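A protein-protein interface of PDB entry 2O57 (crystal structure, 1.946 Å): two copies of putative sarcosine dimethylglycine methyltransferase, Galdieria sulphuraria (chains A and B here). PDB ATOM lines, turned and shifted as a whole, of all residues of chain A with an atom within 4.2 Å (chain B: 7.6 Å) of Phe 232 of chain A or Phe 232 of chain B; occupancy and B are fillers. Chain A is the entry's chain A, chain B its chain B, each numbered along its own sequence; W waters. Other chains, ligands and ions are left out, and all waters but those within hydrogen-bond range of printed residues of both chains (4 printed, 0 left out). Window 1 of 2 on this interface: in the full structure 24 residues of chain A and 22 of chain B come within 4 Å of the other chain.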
ATOM      1  N   TRP A  69      16.182 -19.824  16.735  1.00  0.00           N
ATOM      2  CA  TRP A  69      15.851 -20.345  15.383  1.00  0.00           C
ATOM      3  C   TRP A  69      14.563 -19.689  14.863  1.00  0.00           C
ATOM      4  O   TRP A  69      14.534 -19.167  13.748  1.00  0.00           O
ATOM      5  CB  TRP A  69      15.700 -21.897  15.371  1.00  0.00           C
ATOM      6  CG  TRP A  69      14.943 -22.405  14.154  1.00  0.00           C
ATOM      7  CD1 TRP A  69      15.355 -22.341  12.838  1.00  0.00           C
ATOM      8  CD2 TRP A  69      13.635 -23.016  14.136  1.00  0.00           C
ATOM      9  NE1 TRP A  69      14.378 -22.869  12.017  1.00  0.00           N
ATOM     10  CE2 TRP A  69      13.326 -23.303  12.784  1.00  0.00           C
ATOM     11  CE3 TRP A  69      12.707 -23.358  15.135  1.00  0.00           C
ATOM     12  CZ2 TRP A  69      12.130 -23.900  12.405  1.00  0.00           C
ATOM     13  CZ3 TRP A  69      11.499 -23.953  14.762  1.00  0.00           C
ATOM     14  CH2 TRP A  69      11.222 -24.225  13.395  1.00  0.00           C
ATOM     15  N   GLU A  73      14.089 -17.130  11.627  1.00  0.00           N
ATOM     16  CA  GLU A  73      13.231 -17.412  10.476  1.00  0.00           C
ATOM     17  C   GLU A  73      12.340 -16.177  10.257  1.00  0.00           C
ATOM     18  O   GLU A  73      12.265 -15.656   9.157  1.00  0.00           O
ATOM     19  CB  GLU A  73      12.391 -18.693  10.691  1.00  0.00           C
ATOM     20  CG  GLU A  73      13.245 -20.006  10.815  1.00  0.00           C
ATOM     21  CD  GLU A  73      13.806 -20.489   9.503  1.00  0.00           C
ATOM     22  OE1 GLU A  73      13.383 -19.982   8.431  1.00  0.00           O
ATOM     23  OE2 GLU A  73      14.666 -21.381   9.521  1.00  0.00           O
ATOM     24  N   LEU A 214       0.604 -30.318   9.786  1.00  0.00           N
ATOM     25  CA  LEU A 214       1.083 -29.339   8.810  1.00  0.00           C
ATOM     26  C   LEU A 214       0.103 -29.174   7.648  1.00  0.00           C
ATOM     27  O   LEU A 214      -0.131 -28.051   7.204  1.00  0.00           O
ATOM     28  CB  LEU A 214       2.478 -29.722   8.293  1.00  0.00           C
ATOM     29  CG  LEU A 214       3.643 -29.644   9.293  1.00  0.00           C
ATOM     30  CD1 LEU A 214       4.910 -30.227   8.680  1.00  0.00           C
ATOM     31  CD2 LEU A 214       3.900 -28.150   9.746  1.00  0.00           C
ATOM     32  N   ARG A 230       6.967 -21.428   4.517  1.00  0.00           N
ATOM     33  CA  ARG A 230       7.850 -22.553   4.813  1.00  0.00           C
ATOM     34  C   ARG A 230       7.297 -23.389   5.967  1.00  0.00           C
ATOM     35  O   ARG A 230       6.563 -22.863   6.826  1.00  0.00           O
ATOM     36  CB  ARG A 230       9.259 -22.050   5.134  1.00  0.00           C
ATOM     37  CG  ARG A 230       9.356 -21.104   6.351  1.00  0.00           C
ATOM     38  CD  ARG A 230      10.720 -20.443   6.470  1.00  0.00           C
ATOM     39  NE  ARG A 230      10.796 -19.233   5.633  1.00  0.00           N
ATOM     40  CZ  ARG A 230      11.410 -18.100   5.974  1.00  0.00           C
ATOM     41  NH1 ARG A 230      12.069 -17.975   7.132  1.00  0.00           N
ATOM     42  NH2 ARG A 230      11.384 -17.068   5.144  1.00  0.00           N
ATOM     43  N   THR A 231       7.679 -24.669   6.004  1.00  0.00           N
ATOM     44  CA  THR A 231       7.313 -25.579   7.082  1.00  0.00           C
ATOM     45  C   THR A 231       8.487 -26.467   7.515  1.00  0.00           C
ATOM     46  O   THR A 231       9.478 -26.664   6.756  1.00  0.00           O
ATOM     47  CB  THR A 231       6.084 -26.456   6.729  1.00  0.00           C
ATOM     48  OG1 THR A 231       6.391 -27.355   5.664  1.00  0.00           O
ATOM     49  CG2 THR A 231       4.891 -25.608   6.305  1.00  0.00           C
ATOM     50  N   PHE A 232       8.365 -26.990   8.741  1.00  0.00           N
ATOM     51  CA  PHE A 232       9.409 -27.726   9.410  1.00  0.00           C
ATOM     52  C   PHE A 232       8.714 -28.832  10.189  1.00  0.00           C
ATOM     53  O   PHE A 232       7.652 -28.612  10.791  1.00  0.00           O
ATOM     54  CB  PHE A 232      10.180 -26.809  10.402  1.00  0.00           C
ATOM     55  CG  PHE A 232      10.761 -25.553   9.775  1.00  0.00           C
ATOM     56  CD1 PHE A 232      12.089 -25.518   9.341  1.00  0.00           C
ATOM     57  CD2 PHE A 232       9.991 -24.399   9.632  1.00  0.00           C
ATOM     58  CE1 PHE A 232      12.625 -24.347   8.743  1.00  0.00           C
ATOM     59  CE2 PHE A 232      10.514 -23.249   9.023  1.00  0.00           C
ATOM     60  CZ  PHE A 232      11.824 -23.215   8.589  1.00  0.00           C
ATOM     61  N   SER A 233       9.280 -30.030  10.146  1.00  0.00           N
ATOM     62  CA  SER A 233       8.763 -31.146  10.951  1.00  0.00           C
ATOM     63  C   SER A 233       9.986 -31.723  11.637  1.00  0.00           C
ATOM     64  O   SER A 233      10.961 -32.107  10.961  1.00  0.00           O
ATOM     65  CB  SER A 233       8.053 -32.179  10.060  1.00  0.00           C
ATOM     66  OG  SER A 233       7.752 -33.371  10.790  1.00  0.00           O
ATOM     67  N   ARG A 234       9.968 -31.715  12.968  1.00  0.00           N
ATOM     68  CA  ARG A 234      11.109 -32.191  13.732  1.00  0.00           C
ATOM     69  C   ARG A 234      10.640 -33.251  14.715  1.00  0.00           C
ATOM     70  O   ARG A 234      10.517 -32.940  15.914  1.00  0.00           O
ATOM     71  CB  ARG A 234      11.748 -31.030  14.481  1.00  0.00           C
ATOM     72  CG  ARG A 234      12.317 -29.936  13.538  1.00  0.00           C
ATOM     73  CD  ARG A 234      12.853 -28.774  14.361  1.00  0.00           C
ATOM     74  NE  ARG A 234      13.239 -27.610  13.557  1.00  0.00           N
ATOM     75  CZ  ARG A 234      14.479 -27.394  13.135  1.00  0.00           C
ATOM     76  NH1 ARG A 234      15.474 -28.263  13.428  1.00  0.00           N
ATOM     77  NH2 ARG A 234      14.732 -26.283  12.446  1.00  0.00           N
ATOM     78  N   TRP A 286       6.871 -32.444  15.880  1.00  0.00           N
ATOM     79  CA  TRP A 286       6.819 -31.064  16.341  1.00  0.00           C
ATOM     80  C   TRP A 286       6.939 -30.225  15.090  1.00  0.00           C
ATOM     81  O   TRP A 286       7.958 -30.280  14.419  1.00  0.00           O
ATOM     82  CB  TRP A 286       7.945 -30.755  17.340  1.00  0.00           C
ATOM     83  CG  TRP A 286       7.948 -29.302  17.825  1.00  0.00           C
ATOM     84  CD1 TRP A 286       6.899 -28.625  18.419  1.00  0.00           C
ATOM     85  CD2 TRP A 286       9.025 -28.390  17.751  1.00  0.00           C
ATOM     86  NE1 TRP A 286       7.266 -27.337  18.677  1.00  0.00           N
ATOM     87  CE2 TRP A 286       8.580 -27.167  18.313  1.00  0.00           C
ATOM     88  CE3 TRP A 286      10.347 -28.484  17.282  1.00  0.00           C
ATOM     89  CZ2 TRP A 286       9.403 -26.034  18.410  1.00  0.00           C
ATOM     90  CZ3 TRP A 286      11.176 -27.354  17.391  1.00  0.00           C
ATOM     91  CH2 TRP A 286      10.688 -26.142  17.945  1.00  0.00           C
ATOM     92  N   GLY A 287       5.887 -29.475  14.784  1.00  0.00           N
ATOM     93  CA  GLY A 287       5.769 -28.730  13.533  1.00  0.00           C
ATOM     94  C   GLY A 287       6.123 -27.279  13.711  1.00  0.00           C
ATOM     95  O   GLY A 287       5.965 -26.729  14.792  1.00  0.00           O
ATOM     96  N   GLY A 288       6.620 -26.651  12.651  1.00  0.00           N
ATOM     97  CA  GLY A 288       6.898 -25.211  12.675  1.00  0.00           C
ATOM     98  C   GLY A 288       6.437 -24.664  11.331  1.00  0.00           C
ATOM     99  O   GLY A 288       6.591 -25.351  10.308  1.00  0.00           O
ATOM    100  N   LEU B  49      18.845 -19.240   0.974  1.00  0.00           N
ATOM    101  CA  LEU B  49      17.973 -18.691   1.997  1.00  0.00           C
ATOM    102  C   LEU B  49      18.092 -17.162   1.917  1.00  0.00           C
ATOM    103  O   LEU B  49      19.156 -16.573   2.207  1.00  0.00           O
ATOM    104  CB  LEU B  49      18.437 -19.166   3.387  1.00  0.00           C
ATOM    105  CG  LEU B  49      18.362 -20.662   3.753  1.00  0.00           C
ATOM    106  CD1 LEU B  49      18.793 -20.853   5.227  1.00  0.00           C
ATOM    107  CD2 LEU B  49      16.975 -21.133   3.591  1.00  0.00           C
ATOM    108  N   TRP B  69      23.269 -22.993   7.246  1.00  0.00           N
ATOM    109  CA  TRP B  69      22.079 -23.585   7.853  1.00  0.00           C
ATOM    110  C   TRP B  69      22.145 -25.109   7.867  1.00  0.00           C
ATOM    111  O   TRP B  69      21.958 -25.738   8.924  1.00  0.00           O
ATOM    112  CB  TRP B  69      20.795 -23.149   7.126  1.00  0.00           C
ATOM    113  CG  TRP B  69      19.616 -24.013   7.501  1.00  0.00           C
ATOM    114  CD1 TRP B  69      19.031 -24.138   8.757  1.00  0.00           C
ATOM    115  CD2 TRP B  69      18.889 -24.890   6.637  1.00  0.00           C
ATOM    116  NE1 TRP B  69      17.994 -25.030   8.704  1.00  0.00           N
ATOM    117  CE2 TRP B  69      17.886 -25.511   7.419  1.00  0.00           C
ATOM    118  CE3 TRP B  69      18.980 -25.201   5.274  1.00  0.00           C
ATOM    119  CZ2 TRP B  69      16.973 -26.434   6.874  1.00  0.00           C
ATOM    120  CZ3 TRP B  69      18.089 -26.131   4.730  1.00  0.00           C
ATOM    121  CH2 TRP B  69      17.083 -26.731   5.530  1.00  0.00           C
ATOM    122  N   LEU B  70      22.398 -25.714   6.715  1.00  0.00           N
ATOM    123  CA  LEU B  70      22.430 -27.175   6.630  1.00  0.00           C
ATOM    124  C   LEU B  70      23.559 -27.762   7.472  1.00  0.00           C
ATOM    125  O   LEU B  70      23.392 -28.804   8.139  1.00  0.00           O
ATOM    126  CB  LEU B  70      22.579 -27.661   5.178  1.00  0.00           C
ATOM    127  CG  LEU B  70      22.309 -29.164   4.924  1.00  0.00           C
ATOM    128  CD1 LEU B  70      20.784 -29.464   5.057  1.00  0.00           C
ATOM    129  CD2 LEU B  70      22.829 -29.534   3.521  1.00  0.00           C
ATOM    130  N   GLU B  73      22.399 -27.613  11.147  1.00  0.00           N
ATOM    131  CA  GLU B  73      21.452 -28.703  11.425  1.00  0.00           C
ATOM    132  C   GLU B  73      22.236 -30.003  11.598  1.00  0.00           C
ATOM    133  O   GLU B  73      21.990 -30.757  12.536  1.00  0.00           O
ATOM    134  CB  GLU B  73      20.444 -28.913  10.283  1.00  0.00           C
ATOM    135  CG  GLU B  73      19.458 -27.809  10.033  1.00  0.00           C
ATOM    136  CD  GLU B  73      18.405 -27.660  11.115  1.00  0.00           C
ATOM    137  OE1 GLU B  73      18.169 -28.615  11.888  1.00  0.00           O
ATOM    138  OE2 GLU B  73      17.766 -26.592  11.159  1.00  0.00           O
ATOM    139  N   ILE B 185      20.330 -33.807   3.287  1.00  0.00           N
ATOM    140  CA  ILE B 185      20.128 -33.590   1.838  1.00  0.00           C
ATOM    141  C   ILE B 185      19.170 -32.433   1.632  1.00  0.00           C
ATOM    142  O   ILE B 185      18.314 -32.147   2.497  1.00  0.00           O
ATOM    143  CB  ILE B 185      19.557 -34.853   1.062  1.00  0.00           C
ATOM    144  CG1 ILE B 185      18.188 -35.257   1.598  1.00  0.00           C
ATOM    145  CG2 ILE B 185      20.450 -36.036   1.209  1.00  0.00           C
ATOM    146  CD1 ILE B 185      17.245 -35.807   0.517  1.00  0.00           C
ATOM    147  N   THR B 186      19.317 -31.780   0.492  1.00  0.00           N
ATOM    148  CA  THR B 186      18.373 -30.775   0.027  1.00  0.00           C
ATOM    149  C   THR B 186      18.057 -31.124  -1.428  1.00  0.00           C
ATOM    150  O   THR B 186      18.859 -31.752  -2.114  1.00  0.00           O
ATOM    151  CB  THR B 186      18.936 -29.332   0.081  1.00  0.00           C
ATOM    152  OG1 THR B 186      20.001 -29.171  -0.892  1.00  0.00           O
ATOM    153  CG2 THR B 186      19.399 -28.918   1.524  1.00  0.00           C
ATOM    154  N   ASP B 187      16.869 -30.773  -1.889  1.00  0.00           N
ATOM    155  CA  ASP B 187      16.516 -31.060  -3.300  1.00  0.00           C
ATOM    156  C   ASP B 187      15.312 -30.205  -3.727  1.00  0.00           C
ATOM    157  O   ASP B 187      14.321 -30.123  -2.977  1.00  0.00           O
ATOM    158  CB  ASP B 187      16.169 -32.552  -3.416  1.00  0.00           C
ATOM    159  CG  ASP B 187      16.466 -33.142  -4.760  1.00  0.00           C
ATOM    160  OD1 ASP B 187      17.447 -32.733  -5.452  1.00  0.00           O
ATOM    161  OD2 ASP B 187      15.692 -34.064  -5.128  1.00  0.00           O
ATOM    162  N   MET B 189      11.916 -30.082  -5.431  1.00  0.00           N
ATOM    163  CA  MET B 189      10.969 -31.167  -5.462  1.00  0.00           C
ATOM    164  C   MET B 189       9.547 -30.721  -5.683  1.00  0.00           C
ATOM    165  O   MET B 189       9.244 -29.521  -5.726  1.00  0.00           O
ATOM    166  CB  MET B 189      11.113 -32.091  -4.225  1.00  0.00           C
ATOM    167  CG  MET B 189      10.897 -31.491  -2.830  1.00  0.00           C
ATOM    168  SD  MET B 189      11.499 -32.716  -1.318  1.00  0.00           S
ATOM    169  CE  MET B 189      13.158 -32.943  -1.428  1.00  0.00           C
ATOM    170  N   LEU B 214       9.017 -34.936  -0.263  1.00  0.00           N
ATOM    171  CA  LEU B 214       9.365 -35.283   1.121  1.00  0.00           C
ATOM    172  C   LEU B 214       8.777 -36.639   1.492  1.00  0.00           C
ATOM    173  O   LEU B 214       9.466 -37.449   2.122  1.00  0.00           O
ATOM    174  CB  LEU B 214       8.905 -34.216   2.107  1.00  0.00           C
ATOM    175  CG  LEU B 214       9.611 -32.849   2.042  1.00  0.00           C
ATOM    176  CD1 LEU B 214       8.938 -31.824   2.959  1.00  0.00           C
ATOM    177  CD2 LEU B 214      11.092 -32.995   2.419  1.00  0.00           C
ATOM    178  N   LEU B 229      14.835 -37.823  10.710  1.00  0.00           N
ATOM    179  CA  LEU B 229      15.003 -36.987  11.915  1.00  0.00           C
ATOM    180  C   LEU B 229      14.198 -35.685  11.866  1.00  0.00           C
ATOM    181  O   LEU B 229      13.608 -35.256  12.895  1.00  0.00           O
ATOM    182  CB  LEU B 229      16.506 -36.647  12.134  1.00  0.00           C
ATOM    183  CG  LEU B 229      17.456 -37.859  12.334  1.00  0.00           C
ATOM    184  CD1 LEU B 229      18.893 -37.337  12.530  1.00  0.00           C
ATOM    185  CD2 LEU B 229      17.054 -38.769  13.511  1.00  0.00           C
ATOM    186  N   ARG B 230      14.215 -35.033  10.707  1.00  0.00           N
ATOM    187  CA  ARG B 230      13.539 -33.730  10.516  1.00  0.00           C
ATOM    188  C   ARG B 230      13.479 -33.444   9.032  1.00  0.00           C
ATOM    189  O   ARG B 230      14.322 -33.935   8.278  1.00  0.00           O
ATOM    190  CB  ARG B 230      14.270 -32.601  11.260  1.00  0.00           C
ATOM    191  CG  ARG B 230      15.742 -32.411  10.840  1.00  0.00           C
ATOM    192  CD  ARG B 230      16.522 -31.487  11.765  1.00  0.00           C
ATOM    193  NE  ARG B 230      17.037 -32.211  12.935  1.00  0.00           N
ATOM    194  CZ  ARG B 230      18.182 -31.945  13.547  1.00  0.00           C
ATOM    195  NH1 ARG B 230      18.972 -30.937  13.125  1.00  0.00           N
ATOM    196  NH2 ARG B 230      18.553 -32.697  14.597  1.00  0.00           N
ATOM    197  N   THR B 231      12.494 -32.647   8.632  1.00  0.00           N
ATOM    198  CA  THR B 231      12.288 -32.224   7.254  1.00  0.00           C
ATOM    199  C   THR B 231      11.952 -30.733   7.197  1.00  0.00           C
ATOM    200  O   THR B 231      11.436 -30.145   8.170  1.00  0.00           O
ATOM    201  CB  THR B 231      11.158 -33.002   6.514  1.00  0.00           C
ATOM    202  OG1 THR B 231       9.891 -32.608   7.053  1.00  0.00           O
ATOM    203  CG2 THR B 231      11.338 -34.511   6.629  1.00  0.00           C
ATOM    204  N   PHE B 232      12.245 -30.139   6.044  1.00  0.00           N
ATOM    205  CA  PHE B 232      12.010 -28.730   5.783  1.00  0.00           C
ATOM    206  C   PHE B 232      11.389 -28.561   4.425  1.00  0.00           C
ATOM    207  O   PHE B 232      11.717 -29.286   3.486  1.00  0.00           O
ATOM    208  CB  PHE B 232      13.327 -27.946   5.822  1.00  0.00           C
ATOM    209  CG  PHE B 232      14.141 -28.225   7.045  1.00  0.00           C
ATOM    210  CD1 PHE B 232      14.019 -27.417   8.183  1.00  0.00           C
ATOM    211  CD2 PHE B 232      15.025 -29.306   7.074  1.00  0.00           C
ATOM    212  CE1 PHE B 232      14.789 -27.683   9.349  1.00  0.00           C
ATOM    213  CE2 PHE B 232      15.784 -29.586   8.222  1.00  0.00           C
ATOM    214  CZ  PHE B 232      15.671 -28.777   9.359  1.00  0.00           C
ATOM    215  N   SER B 233      10.510 -27.582   4.313  1.00  0.00           N
ATOM    216  CA  SER B 233       9.895 -27.282   3.025  1.00  0.00           C
ATOM    217  C   SER B 233       9.877 -25.792   2.884  1.00  0.00           C
ATOM    218  O   SER B 233       9.277 -25.091   3.700  1.00  0.00           O
ATOM    219  CB  SER B 233       8.493 -27.890   2.924  1.00  0.00           C
ATOM    220  OG  SER B 233       7.931 -27.620   1.642  1.00  0.00           O
ATOM    221  N   ARG B 234      10.618 -25.299   1.902  1.00  0.00           N
ATOM    222  CA  ARG B 234      10.757 -23.859   1.742  1.00  0.00           C
ATOM    223  C   ARG B 234      10.360 -23.418   0.338  1.00  0.00           C
ATOM    224  O   ARG B 234      11.235 -23.115  -0.474  1.00  0.00           O
ATOM    225  CB  ARG B 234      12.200 -23.452   2.035  1.00  0.00           C
ATOM    226  CG  ARG B 234      12.605 -23.595   3.462  1.00  0.00           C
ATOM    227  CD  ARG B 234      14.104 -23.443   3.517  1.00  0.00           C
ATOM    228  NE  ARG B 234      14.724 -23.753   4.810  1.00  0.00           N
ATOM    229  CZ  ARG B 234      14.702 -22.944   5.863  1.00  0.00           C
ATOM    230  NH1 ARG B 234      13.998 -21.799   5.807  1.00  0.00           N
ATOM    231  NH2 ARG B 234      15.352 -23.301   6.983  1.00  0.00           N
ATOM    232  N   PRO B 235       9.051 -23.384   0.044  1.00  0.00           N
ATOM    233  CA  PRO B 235       8.657 -22.914  -1.267  1.00  0.00           C
ATOM    234  C   PRO B 235       8.983 -21.419  -1.473  1.00  0.00           C
ATOM    235  O   PRO B 235       9.257 -21.013  -2.603  1.00  0.00           O
ATOM    236  CB  PRO B 235       7.148 -23.169  -1.299  1.00  0.00           C
ATOM    237  CG  PRO B 235       6.736 -23.171   0.163  1.00  0.00           C
ATOM    238  CD  PRO B 235       7.878 -23.802   0.860  1.00  0.00           C
ATOM    239  N   ASP B 236       9.046 -20.632  -0.400  1.00  0.00           N
ATOM    240  CA  ASP B 236       9.510 -19.241  -0.561  1.00  0.00           C
ATOM    241  C   ASP B 236      10.963 -19.183  -1.121  1.00  0.00           C
ATOM    242  O   ASP B 236      11.258 -18.395  -2.055  1.00  0.00           O
ATOM    243  CB  ASP B 236       9.349 -18.444   0.728  1.00  0.00           C
ATOM    244  CG  ASP B 236      10.142 -19.032   1.928  1.00  0.00           C
ATOM    245  OD1 ASP B 236      10.753 -20.151   1.870  1.00  0.00           O
ATOM    246  OD2 ASP B 236      10.137 -18.331   2.936  1.00  0.00           O
ATOM    247  N   THR B 285       8.367 -27.330  -4.302  1.00  0.00           N
ATOM    248  CA  THR B 285       9.014 -26.799  -3.104  1.00  0.00           C
ATOM    249  C   THR B 285      10.501 -27.074  -3.161  1.00  0.00           C
ATOM    250  O   THR B 285      10.990 -27.775  -4.088  1.00  0.00           O
ATOM    251  CB  THR B 285       8.368 -27.328  -1.768  1.00  0.00           C
ATOM    252  OG1 THR B 285       8.905 -26.582  -0.671  1.00  0.00           O
ATOM    253  CG2 THR B 285       8.674 -28.850  -1.522  1.00  0.00           C
ATOM    254  N   TRP B 286      11.230 -26.485  -2.219  1.00  0.00           N
ATOM    255  CA  TRP B 286      12.639 -26.814  -2.026  1.00  0.00           C
ATOM    256  C   TRP B 286      12.683 -27.470  -0.666  1.00  0.00           C
ATOM    257  O   TRP B 286      12.392 -26.811   0.375  1.00  0.00           O
ATOM    258  CB  TRP B 286      13.540 -25.568  -2.060  1.00  0.00           C
ATOM    259  CG  TRP B 286      15.025 -25.889  -1.807  1.00  0.00           C
ATOM    260  CD1 TRP B 286      15.827 -26.762  -2.524  1.00  0.00           C
ATOM    261  CD2 TRP B 286      15.846 -25.349  -0.781  1.00  0.00           C
ATOM    262  NE1 TRP B 286      17.078 -26.794  -1.987  1.00  0.00           N
ATOM    263  CE2 TRP B 286      17.134 -25.928  -0.926  1.00  0.00           C
ATOM    264  CE3 TRP B 286      15.640 -24.406   0.243  1.00  0.00           C
ATOM    265  CZ2 TRP B 286      18.199 -25.595  -0.090  1.00  0.00           C
ATOM    266  CZ3 TRP B 286      16.695 -24.092   1.069  1.00  0.00           C
ATOM    267  CH2 TRP B 286      17.942 -24.705   0.927  1.00  0.00           C
ATOM    268  N   GLY B 287      12.978 -28.766  -0.676  1.00  0.00           N
ATOM    269  CA  GLY B 287      12.887 -29.554   0.544  1.00  0.00           C
ATOM    270  C   GLY B 287      14.254 -29.946   1.054  1.00  0.00           C
ATOM    271  O   GLY B 287      15.273 -29.919   0.323  1.00  0.00           O
ATOM    272  N   GLY B 288      14.292 -30.241   2.340  1.00  0.00           N
ATOM    273  CA  GLY B 288      15.516 -30.610   3.026  1.00  0.00           C
ATOM    274  C   GLY B 288      15.161 -31.664   4.086  1.00  0.00           C
ATOM    275  O   GLY B 288      14.057 -31.638   4.660  1.00  0.00           O
ATOM    276  N   MET B 289      16.092 -32.581   4.339  1.00  0.00           N
ATOM    277  CA  MET B 289      15.876 -33.678   5.278  1.00  0.00           C
ATOM    278  C   MET B 289      17.168 -34.102   5.899  1.00  0.00           C
ATOM    279  O   MET B 289      18.207 -34.024   5.261  1.00  0.00           O
ATOM    280  CB  MET B 289      15.266 -34.879   4.540  1.00  0.00           C
ATOM    281  CG  MET B 289      14.227 -34.437   3.546  1.00  0.00           C
ATOM    282  SD  MET B 289      13.697 -35.798   2.366  1.00  0.00           S
ATOM    283  CE  MET B 289      12.526 -36.856   3.593  1.00  0.00           C
ATOM    284  N   LEU B 290      17.102 -34.549   7.157  1.00  0.00           N
ATOM    285  CA  LEU B 290      18.188 -35.268   7.798  1.00  0.00           C
ATOM    286  C   LEU B 290      17.664 -36.665   8.143  1.00  0.00           C
ATOM    287  O   LEU B 290      16.500 -36.800   8.612  1.00  0.00           O
ATOM    288  CB  LEU B 290      18.706 -34.537   9.065  1.00  0.00           C
ATOM    289  CG  LEU B 290      19.775 -33.458   8.780  1.00  0.00           C
ATOM    290  CD1 LEU B 290      19.190 -32.301   8.029  1.00  0.00           C
ATOM    291  CD2 LEU B 290      20.418 -32.960  10.080  1.00  0.00           C
HETATM  292  O   HOH W   1       5.915 -25.391   3.058  1.00  0.00           O
HETATM  293  O   HOH W   2      15.340 -30.856  15.434  1.00  0.00           O
HETATM  294  O   HOH W   3      13.147 -20.096   3.251  1.00  0.00           O
HETATM  295  O   HOH W   4       8.380 -30.097   6.521  1.00  0.00           O
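Printed residues of chain B within 4 Å of Arg 230 of chain A: Ser 233, Arg 234 and Asp 236.
Of chain B, only Thr 231, Phe 232 and Arg 234 come within 4 Å of Phe 232 of chain A.
Leu 49 of chain B touches none of the printed residues of chain A.
Printed residues of chain A within 4 Å of Arg 230 of chain B: Ser 233 (3.1 Å) and Arg 234 (3.8 Å).
Printed residues of chain A within 4 Å of Phe 232 of chain B: Thr 231, Phe 232 and Arg 234.
Printed residues of chain A within 4 Å of Arg 234 of chain B: Glu 73 (3.3 Å), Arg 230 (3.6 Å) and Phe 232 (3.4 Å).
The nearest residue of chain B that does not touch Phe 232 of chain A is Ser 233 of chain B (5.0 Å).
Of the 23 printed residues of chain B, 7 touch a printed residue of chain A.
Of the 11 printed residues of chain A, 6 touch a printed residue of chain B.
Hydrophobic or aromatic side chains of chain A that line the printed part of chain B: Phe 232.
Among the printed residues, 14 pairs touch across the chains.
Among the printed residues, Asp or Glu carboxylates within 4 Å of a Lys or Arg side-chain nitrogen of the other chain: Glu 73 of chain A with Arg 234 of chain B (3.3 Å), Arg 230 of chain A with Asp 236 of chain B (2.8 Å) and Arg 234 of chain A with Glu 73 of chain B (3.1 Å).
Water W3 lies within hydrogen-bond range of the side-chain carboxylate (OD1) of Asp 236 of chain B (2.8 Å), the guanidinium group (NH1) of Arg 234 of chain B (3.2 Å) and the guanidinium group (NE) of Arg 230 of chain A (3.5 Å).
Water W4 lies within hydrogen-bond range of the side-chain hydroxyl (OG1) of Thr 231 of chain B (3.0 Å) and the side-chain hydroxyl (OG1) of Thr 231 of chain A (3.5 Å).
Water W2 lies within hydrogen-bond range of the guanidinium group of Arg 234 of chain A (3.3 Å) and the guanidinium group of Arg 230 of chain B (3.3 Å).
Water W1 bridges OG1 of Thr 231 of chain A and OG of Ser 233 of chain B.
Arg 230 of chain A touches Arg 234 of chain B, and with the chains exchanged Arg 234 of chain A touches Arg 230 of chain B.
Thr 231 of chain A touches Phe 232 of chain B, and with the chains exchanged Phe 232 of chain A touches Thr 231 of chain B.
Thr 231 of chain A touches Ser 233 of chain B, and with the chains exchanged Ser 233 of chain A touches Thr 231 of chain B.
Phe 232 of chain A touches Arg 234 of chain B, and with the chains exchanged Arg 234 of chain A touches Phe 232 of chain B.
NH1 of Arg 234 of chain B lies within salt-bridge range of OE1 of Glu 73 of chain A, 3.3 Å away.
The side-chain carboxylate (OD2) of Asp 236 of chain B lies within salt-bridge range of the guanidinium group (NH2) of Arg 230 of chain A (2.8 Å).
O of Thr 231 of chain A is in hydrogen-bond range of N of Ser 233 of chain B (2.8 Å).
O of Ser 233 of chain A is in hydrogen-bond range of N of Thr 231 of chain B (2.8 Å).
The guanidinium group of Arg 234 of chain A lies within salt-bridge range of the side-chain carboxylate of Glu 73 of chain B, at 3.1 Å.
The indole nitrogen (NE1) of Trp 69 of chain A lies within hydrogen-bond range of the side-chain carboxylate (OE2) of Glu 73 of chain A.
OE1 of Glu 73 of chain A is in salt-bridge range of NH1 of Arg 230 of chain A (2.7 Å).
The backbone carbonyl oxygen of Trp 286 of chain A is in hydrogen-bond range of the backbone NH of Arg 234 of chain A, 2.9 Å away.
OG1 of Thr 285 of chain B lies within hydrogen-bond range of N of Arg 234 of chain B (3.3 Å).
O of Trp 286 of chain B sits at hydrogen-bond distance from N of Arg 234 of chain B (2.8 Å).
Arg 230 of chain A touches Ser 233 of chain B.
Arg 230 of chain A touches Arg 234 of chain B.
Thr 231 of chain A touches Phe 232 of chain B (O to CA, 3.4 Å).
Thr 231 of chain B touches Phe 232 of chain A.
Phe 232 of chain A touches Phe 232 of chain B (CD1 to CD1, 2.9 Å).
CE1 of Phe 232 of chain A touches NH2 of Arg 234 of chain B, 3.4 Å away.
Arg 230 of chain B touches Ser 233 of chain A.
Arg 234 of chain A touches Arg 230 of chain B.
NH2 of Arg 234 of chain A touches CE1 of Phe 232 of chain B (3.4 Å).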
